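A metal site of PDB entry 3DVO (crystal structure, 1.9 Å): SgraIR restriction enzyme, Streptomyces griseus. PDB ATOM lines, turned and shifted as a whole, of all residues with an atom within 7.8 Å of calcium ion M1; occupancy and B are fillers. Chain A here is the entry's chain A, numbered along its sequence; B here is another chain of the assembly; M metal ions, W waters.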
ATOM      1  N   ASP A  99       7.130  22.107  -0.949  1.00  0.00           N
ATOM      2  CA  ASP A  99       6.788  20.834  -0.289  1.00  0.00           C
ATOM      3  C   ASP A  99       6.989  20.884   1.255  1.00  0.00           C
ATOM      4  O   ASP A  99       6.143  20.451   2.031  1.00  0.00           O
ATOM      5  CB  ASP A  99       7.573  19.674  -0.921  1.00  0.00           C
ATOM      6  CG  ASP A  99       6.976  19.197  -2.274  1.00  0.00           C
ATOM      7  OD1 ASP A  99       5.971  19.782  -2.788  1.00  0.00           O
ATOM      8  OD2 ASP A  99       7.537  18.206  -2.826  1.00  0.00           O
ATOM      9  N   GLU A 102       4.315  22.893   2.895  1.00  0.00           N
ATOM     10  CA  GLU A 102       3.116  22.068   2.973  1.00  0.00           C
ATOM     11  C   GLU A 102       3.207  20.934   3.998  1.00  0.00           C
ATOM     12  O   GLU A 102       2.280  20.663   4.758  1.00  0.00           O
ATOM     13  CB  GLU A 102       2.822  21.443   1.619  1.00  0.00           C
ATOM     14  CG  GLU A 102       1.491  20.736   1.604  1.00  0.00           C
ATOM     15  CD  GLU A 102       1.355  19.832   0.418  1.00  0.00           C
ATOM     16  OE1 GLU A 102       2.081  20.037  -0.593  1.00  0.00           O
ATOM     17  OE2 GLU A 102       0.519  18.914   0.498  1.00  0.00           O
ATOM     18  N   ILE A 103       4.353  20.267   4.010  1.00  0.00           N
ATOM     19  CA  ILE A 103       4.532  19.171   4.935  1.00  0.00           C
ATOM     20  C   ILE A 103       4.556  19.614   6.390  1.00  0.00           C
ATOM     21  O   ILE A 103       3.838  19.046   7.224  1.00  0.00           O
ATOM     22  CB  ILE A 103       5.770  18.362   4.567  1.00  0.00           C
ATOM     23  CG1 ILE A 103       5.524  17.632   3.231  1.00  0.00           C
ATOM     24  CG2 ILE A 103       6.082  17.395   5.664  1.00  0.00           C
ATOM     25  CD1 ILE A 103       6.813  17.304   2.431  1.00  0.00           C
ATOM     26  N   SER A 106       1.035  20.912   7.755  1.00  0.00           N
ATOM     27  CA  SER A 106       0.040  19.852   7.987  1.00  0.00           C
ATOM     28  C   SER A 106       0.428  18.950   9.176  1.00  0.00           C
ATOM     29  O   SER A 106      -0.438  18.367   9.833  1.00  0.00           O
ATOM     30  CB  SER A 106      -0.220  19.057   6.719  1.00  0.00           C
ATOM     31  OG  SER A 106       1.014  18.729   6.111  1.00  0.00           O
ATOM     32  N   LEU A 147      -5.579  15.104   6.869  1.00  0.00           N
ATOM     33  CA  LEU A 147      -5.138  14.344   5.702  1.00  0.00           C
ATOM     34  C   LEU A 147      -4.336  15.175   4.708  1.00  0.00           C
ATOM     35  O   LEU A 147      -4.886  15.877   3.860  1.00  0.00           O
ATOM     36  CB  LEU A 147      -6.333  13.707   4.996  1.00  0.00           C
ATOM     37  CG  LEU A 147      -7.298  12.931   5.883  1.00  0.00           C
ATOM     38  CD1 LEU A 147      -8.494  12.438   5.042  1.00  0.00           C
ATOM     39  CD2 LEU A 147      -6.595  11.766   6.508  1.00  0.00           C
ATOM     40  N   ASN A 148      -3.018  15.113   4.834  1.00  0.00           N
ATOM     41  CA  ASN A 148      -2.161  15.578   3.760  1.00  0.00           C
ATOM     42  C   ASN A 148      -2.398  14.696   2.530  1.00  0.00           C
ATOM     43  O   ASN A 148      -2.076  13.489   2.526  1.00  0.00           O
ATOM     44  CB  ASN A 148      -0.718  15.482   4.241  1.00  0.00           C
ATOM     45  CG  ASN A 148       0.254  15.877   3.191  1.00  0.00           C
ATOM     46  OD1 ASN A 148      -0.118  16.055   2.049  1.00  0.00           O
ATOM     47  ND2 ASN A 148       1.518  16.025   3.566  1.00  0.00           N
ATOM     48  N   LEU A 149      -2.950  15.286   1.470  1.00  0.00           N
ATOM     49  CA  LEU A 149      -3.330  14.531   0.269  1.00  0.00           C
ATOM     50  C   LEU A 149      -2.178  14.433  -0.722  1.00  0.00           C
ATOM     51  O   LEU A 149      -1.445  15.383  -0.891  1.00  0.00           O
ATOM     52  CB  LEU A 149      -4.527  15.206  -0.399  1.00  0.00           C
ATOM     53  CG  LEU A 149      -5.750  15.275   0.524  1.00  0.00           C
ATOM     54  CD1 LEU A 149      -6.946  15.894  -0.162  1.00  0.00           C
ATOM     55  CD2 LEU A 149      -6.097  13.869   0.967  1.00  0.00           C
ATOM     56  N   PRO A 150      -2.032  13.285  -1.400  1.00  0.00           N
ATOM     57  CA  PRO A 150      -0.867  13.058  -2.271  1.00  0.00           C
ATOM     58  C   PRO A 150      -0.940  13.713  -3.655  1.00  0.00           C
ATOM     59  O   PRO A 150      -2.005  14.122  -4.113  1.00  0.00           O
ATOM     60  CB  PRO A 150      -0.883  11.543  -2.437  1.00  0.00           C
ATOM     61  CG  PRO A 150      -2.308  11.226  -2.509  1.00  0.00           C
ATOM     62  CD  PRO A 150      -2.962  12.144  -1.477  1.00  0.00           C
ATOM     63  N   ARG A 151       0.199  13.783  -4.332  1.00  0.00           N
ATOM     64  CA  ARG A 151       0.178  14.157  -5.742  1.00  0.00           C
ATOM     65  C   ARG A 151      -0.706  13.168  -6.517  1.00  0.00           C
ATOM     66  O   ARG A 151      -0.731  11.979  -6.219  1.00  0.00           O
ATOM     67  CB  ARG A 151       1.590  14.240  -6.318  1.00  0.00           C
ATOM     68  CG  ARG A 151       2.382  15.479  -5.846  1.00  0.00           C
ATOM     69  CD  ARG A 151       3.732  15.614  -6.539  1.00  0.00           C
ATOM     70  NE  ARG A 151       4.145  17.011  -6.638  1.00  0.00           N
ATOM     71  CZ  ARG A 151       4.878  17.627  -5.722  1.00  0.00           C
ATOM     72  NH1 ARG A 151       5.300  16.971  -4.654  1.00  0.00           N
ATOM     73  NH2 ARG A 151       5.202  18.917  -5.880  1.00  0.00           N
ATOM     74  N   THR A 185      -7.514  18.045  -6.461  1.00  0.00           N
ATOM     75  CA  THR A 185      -7.441  17.937  -4.993  1.00  0.00           C
ATOM     76  C   THR A 185      -6.891  19.211  -4.316  1.00  0.00           C
ATOM     77  O   THR A 185      -6.150  19.964  -4.926  1.00  0.00           O
ATOM     78  CB  THR A 185      -6.561  16.712  -4.580  1.00  0.00           C
ATOM     79  OG1 THR A 185      -6.546  16.581  -3.151  1.00  0.00           O
ATOM     80  CG2 THR A 185      -5.151  16.885  -5.083  1.00  0.00           C
ATOM     81  N   PRO A 186      -7.274  19.457  -3.062  1.00  0.00           N
ATOM     82  CA  PRO A 186      -6.614  20.499  -2.264  1.00  0.00           C
ATOM     83  C   PRO A 186      -5.388  19.856  -1.668  1.00  0.00           C
ATOM     84  O   PRO A 186      -5.291  18.633  -1.809  1.00  0.00           O
ATOM     85  CB  PRO A 186      -7.633  20.766  -1.150  1.00  0.00           C
ATOM     86  CG  PRO A 186      -8.302  19.471  -1.005  1.00  0.00           C
ATOM     87  CD  PRO A 186      -8.508  18.994  -2.390  1.00  0.00           C
ATOM     88  N   ASP A 187      -4.470  20.588  -1.046  1.00  0.00           N
ATOM     89  CA  ASP A 187      -3.293  19.908  -0.499  1.00  0.00           C
ATOM     90  C   ASP A 187      -3.698  19.108   0.734  1.00  0.00           C
ATOM     91  O   ASP A 187      -3.064  18.123   1.079  1.00  0.00           O
ATOM     92  CB  ASP A 187      -2.207  20.877  -0.061  1.00  0.00           C
ATOM     93  CG  ASP A 187      -1.556  21.584  -1.217  1.00  0.00           C
ATOM     94  OD1 ASP A 187      -0.859  20.921  -2.022  1.00  0.00           O
ATOM     95  OD2 ASP A 187      -1.722  22.810  -1.317  1.00  0.00           O
ATOM     96  N   LEU A 188      -4.735  19.564   1.416  1.00  0.00           N
ATOM     97  CA  LEU A 188      -5.058  18.963   2.698  1.00  0.00           C
ATOM     98  C   LEU A 188      -6.541  18.941   2.928  1.00  0.00           C
ATOM     99  O   LEU A 188      -7.242  19.851   2.493  1.00  0.00           O
ATOM    100  CB  LEU A 188      -4.350  19.723   3.821  1.00  0.00           C
ATOM    101  CG  LEU A 188      -4.639  19.345   5.277  1.00  0.00           C
ATOM    102  CD1 LEU A 188      -3.333  19.407   6.057  1.00  0.00           C
ATOM    103  CD2 LEU A 188      -5.681  20.268   5.876  1.00  0.00           C
ATOM    104  N   SER A 219       1.796  11.209   5.554  1.00  0.00           N
ATOM    105  CA  SER A 219       1.547  11.181   4.125  1.00  0.00           C
ATOM    106  C   SER A 219       0.684  10.000   3.689  1.00  0.00           C
ATOM    107  O   SER A 219       0.116  10.029   2.611  1.00  0.00           O
ATOM    108  CB  SER A 219       2.844  11.214   3.326  1.00  0.00           C
ATOM    109  OG  SER A 219       3.608  10.064   3.559  1.00  0.00           O
ATOM    110  N   PHE A 240      -1.887  25.170   0.237  1.00  0.00           N
ATOM    111  CA  PHE A 240      -0.718  25.899   0.709  1.00  0.00           C
ATOM    112  C   PHE A 240       0.020  26.461  -0.497  1.00  0.00           C
ATOM    113  O   PHE A 240       0.270  25.723  -1.442  1.00  0.00           O
ATOM    114  CB  PHE A 240       0.237  24.960   1.451  1.00  0.00           C
ATOM    115  CG  PHE A 240      -0.341  24.362   2.709  1.00  0.00           C
ATOM    116  CD1 PHE A 240      -0.293  25.052   3.910  1.00  0.00           C
ATOM    117  CD2 PHE A 240      -0.926  23.113   2.691  1.00  0.00           C
ATOM    118  CE1 PHE A 240      -0.811  24.506   5.068  1.00  0.00           C
ATOM    119  CE2 PHE A 240      -1.464  22.552   3.864  1.00  0.00           C
ATOM    120  CZ  PHE A 240      -1.397  23.254   5.039  1.00  0.00           C
ATOM    121  P    DA B   7      -1.250  16.693  -9.642  1.00  0.00           P
ATOM    122  OP1  DA B   7      -2.164  16.198  -8.597  1.00  0.00           O
ATOM    123  OP2  DA B   7      -1.760  17.137 -10.952  1.00  0.00           O
ATOM    124  O5'  DA B   7      -0.363  17.888  -9.047  1.00  0.00           O
ATOM    125  C5'  DA B   7       0.325  17.551  -7.853  1.00  0.00           C
ATOM    126  C4'  DA B   7       1.267  18.650  -7.418  1.00  0.00           C
ATOM    127  O4'  DA B   7       2.434  18.573  -8.271  1.00  0.00           O
ATOM    128  C3'  DA B   7       0.723  20.075  -7.520  1.00  0.00           C
ATOM    129  O3'  DA B   7       1.228  20.756  -6.398  1.00  0.00           O
ATOM    130  C2'  DA B   7       1.333  20.574  -8.832  1.00  0.00           C
ATOM    131  C1'  DA B   7       2.682  19.847  -8.839  1.00  0.00           C
ATOM    132  N9   DA B   7       3.327  19.696 -10.133  1.00  0.00           N
ATOM    133  C8   DA B   7       2.771  19.621 -11.385  1.00  0.00           C
ATOM    134  N7   DA B   7       3.678  19.470 -12.326  1.00  0.00           N
ATOM    135  C5   DA B   7       4.910  19.432 -11.660  1.00  0.00           C
ATOM    136  C6   DA B   7       6.268  19.312 -12.071  1.00  0.00           C
ATOM    137  N6   DA B   7       6.697  19.184 -13.326  1.00  0.00           N
ATOM    138  N1   DA B   7       7.220  19.344 -11.112  1.00  0.00           N
ATOM    139  C2   DA B   7       6.830  19.459  -9.848  1.00  0.00           C
ATOM    140  N3   DA B   7       5.592  19.586  -9.348  1.00  0.00           N
ATOM    141  C4   DA B   7       4.682  19.568 -10.316  1.00  0.00           C
ATOM    142  P    DC B   8       0.913  22.260  -5.915  1.00  0.00           P
ATOM    143  OP1  DC B   8       0.262  22.063  -4.615  1.00  0.00           O
ATOM    144  OP2  DC B   8       0.278  23.108  -6.930  1.00  0.00           O
ATOM    145  O5'  DC B   8       2.418  22.757  -5.655  1.00  0.00           O
ATOM    146  C5'  DC B   8       3.241  22.032  -4.770  1.00  0.00           C
ATOM    147  C4'  DC B   8       4.683  22.538  -4.805  1.00  0.00           C
ATOM    148  O4'  DC B   8       5.369  21.898  -5.912  1.00  0.00           O
ATOM    149  C3'  DC B   8       4.867  24.042  -5.046  1.00  0.00           C
ATOM    150  O3'  DC B   8       4.900  24.761  -3.819  1.00  0.00           O
ATOM    151  C2'  DC B   8       6.252  24.105  -5.676  1.00  0.00           C
ATOM    152  C1'  DC B   8       6.307  22.812  -6.487  1.00  0.00           C
ATOM    153  N1   DC B   8       6.023  22.926  -7.944  1.00  0.00           N
ATOM    154  C2   DC B   8       7.099  23.018  -8.825  1.00  0.00           C
ATOM    155  O2   DC B   8       8.245  23.064  -8.373  1.00  0.00           O
ATOM    156  N3   DC B   8       6.872  23.103 -10.158  1.00  0.00           N
ATOM    157  C4   DC B   8       5.628  23.086 -10.625  1.00  0.00           C
ATOM    158  N4   DC B   8       5.471  23.164 -11.954  1.00  0.00           N
ATOM    159  C5   DC B   8       4.512  22.982  -9.727  1.00  0.00           C
ATOM    160  C6   DC B   8       4.746  22.892  -8.414  1.00  0.00           C
HETATM  161 CA    CA M   1       0.731  16.423  -0.362  1.00  0.00          CA
HETATM  162 CA    CA M   2      -0.150  23.687  -2.880  1.00  0.00          CA
HETATM  163  O   HOH W   1      -0.532  18.225  -1.984  1.00  0.00           O
HETATM  164  O   HOH W   2       2.693  17.242  -2.151  1.00  0.00           O
HETATM  165  O   HOH W   3       1.932  13.715   0.232  1.00  0.00           O
HETATM  166  O   HOH W   4       3.184  16.273   0.432  1.00  0.00           O
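Calcium ion M1 is bound by O of Leu 149, 2.5 Å away. Calcium ion M1 is bound by water W4, at 2.6 Å. OD1 of Asn 148 is bound to calcium ion M1. OE2 of Glu 102 is bound to calcium ion M1 (2.6 Å). Water W1 is bound to calcium ion M1, at 2.7 Å. Calcium ion M1 is bound by water W2 (2.8 Å). Slightly farther from calcium ion M1 lies water W3 (3.0 Å).
Water W1 lies within hydrogen-bond range of OD1 of Asp 187 (2.7 Å) and OE1 of Glu 102 (3.5 Å).
The backbone carbonyl oxygen of Glu 102 is in hydrogen-bond range of the side-chain hydroxyl of Ser 106 (2.7 Å). The backbone NH (N) of Leu 149 sits at hydrogen-bond distance from the backbone carbonyl oxygen (O) of Asp 187, at 2.9 Å.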
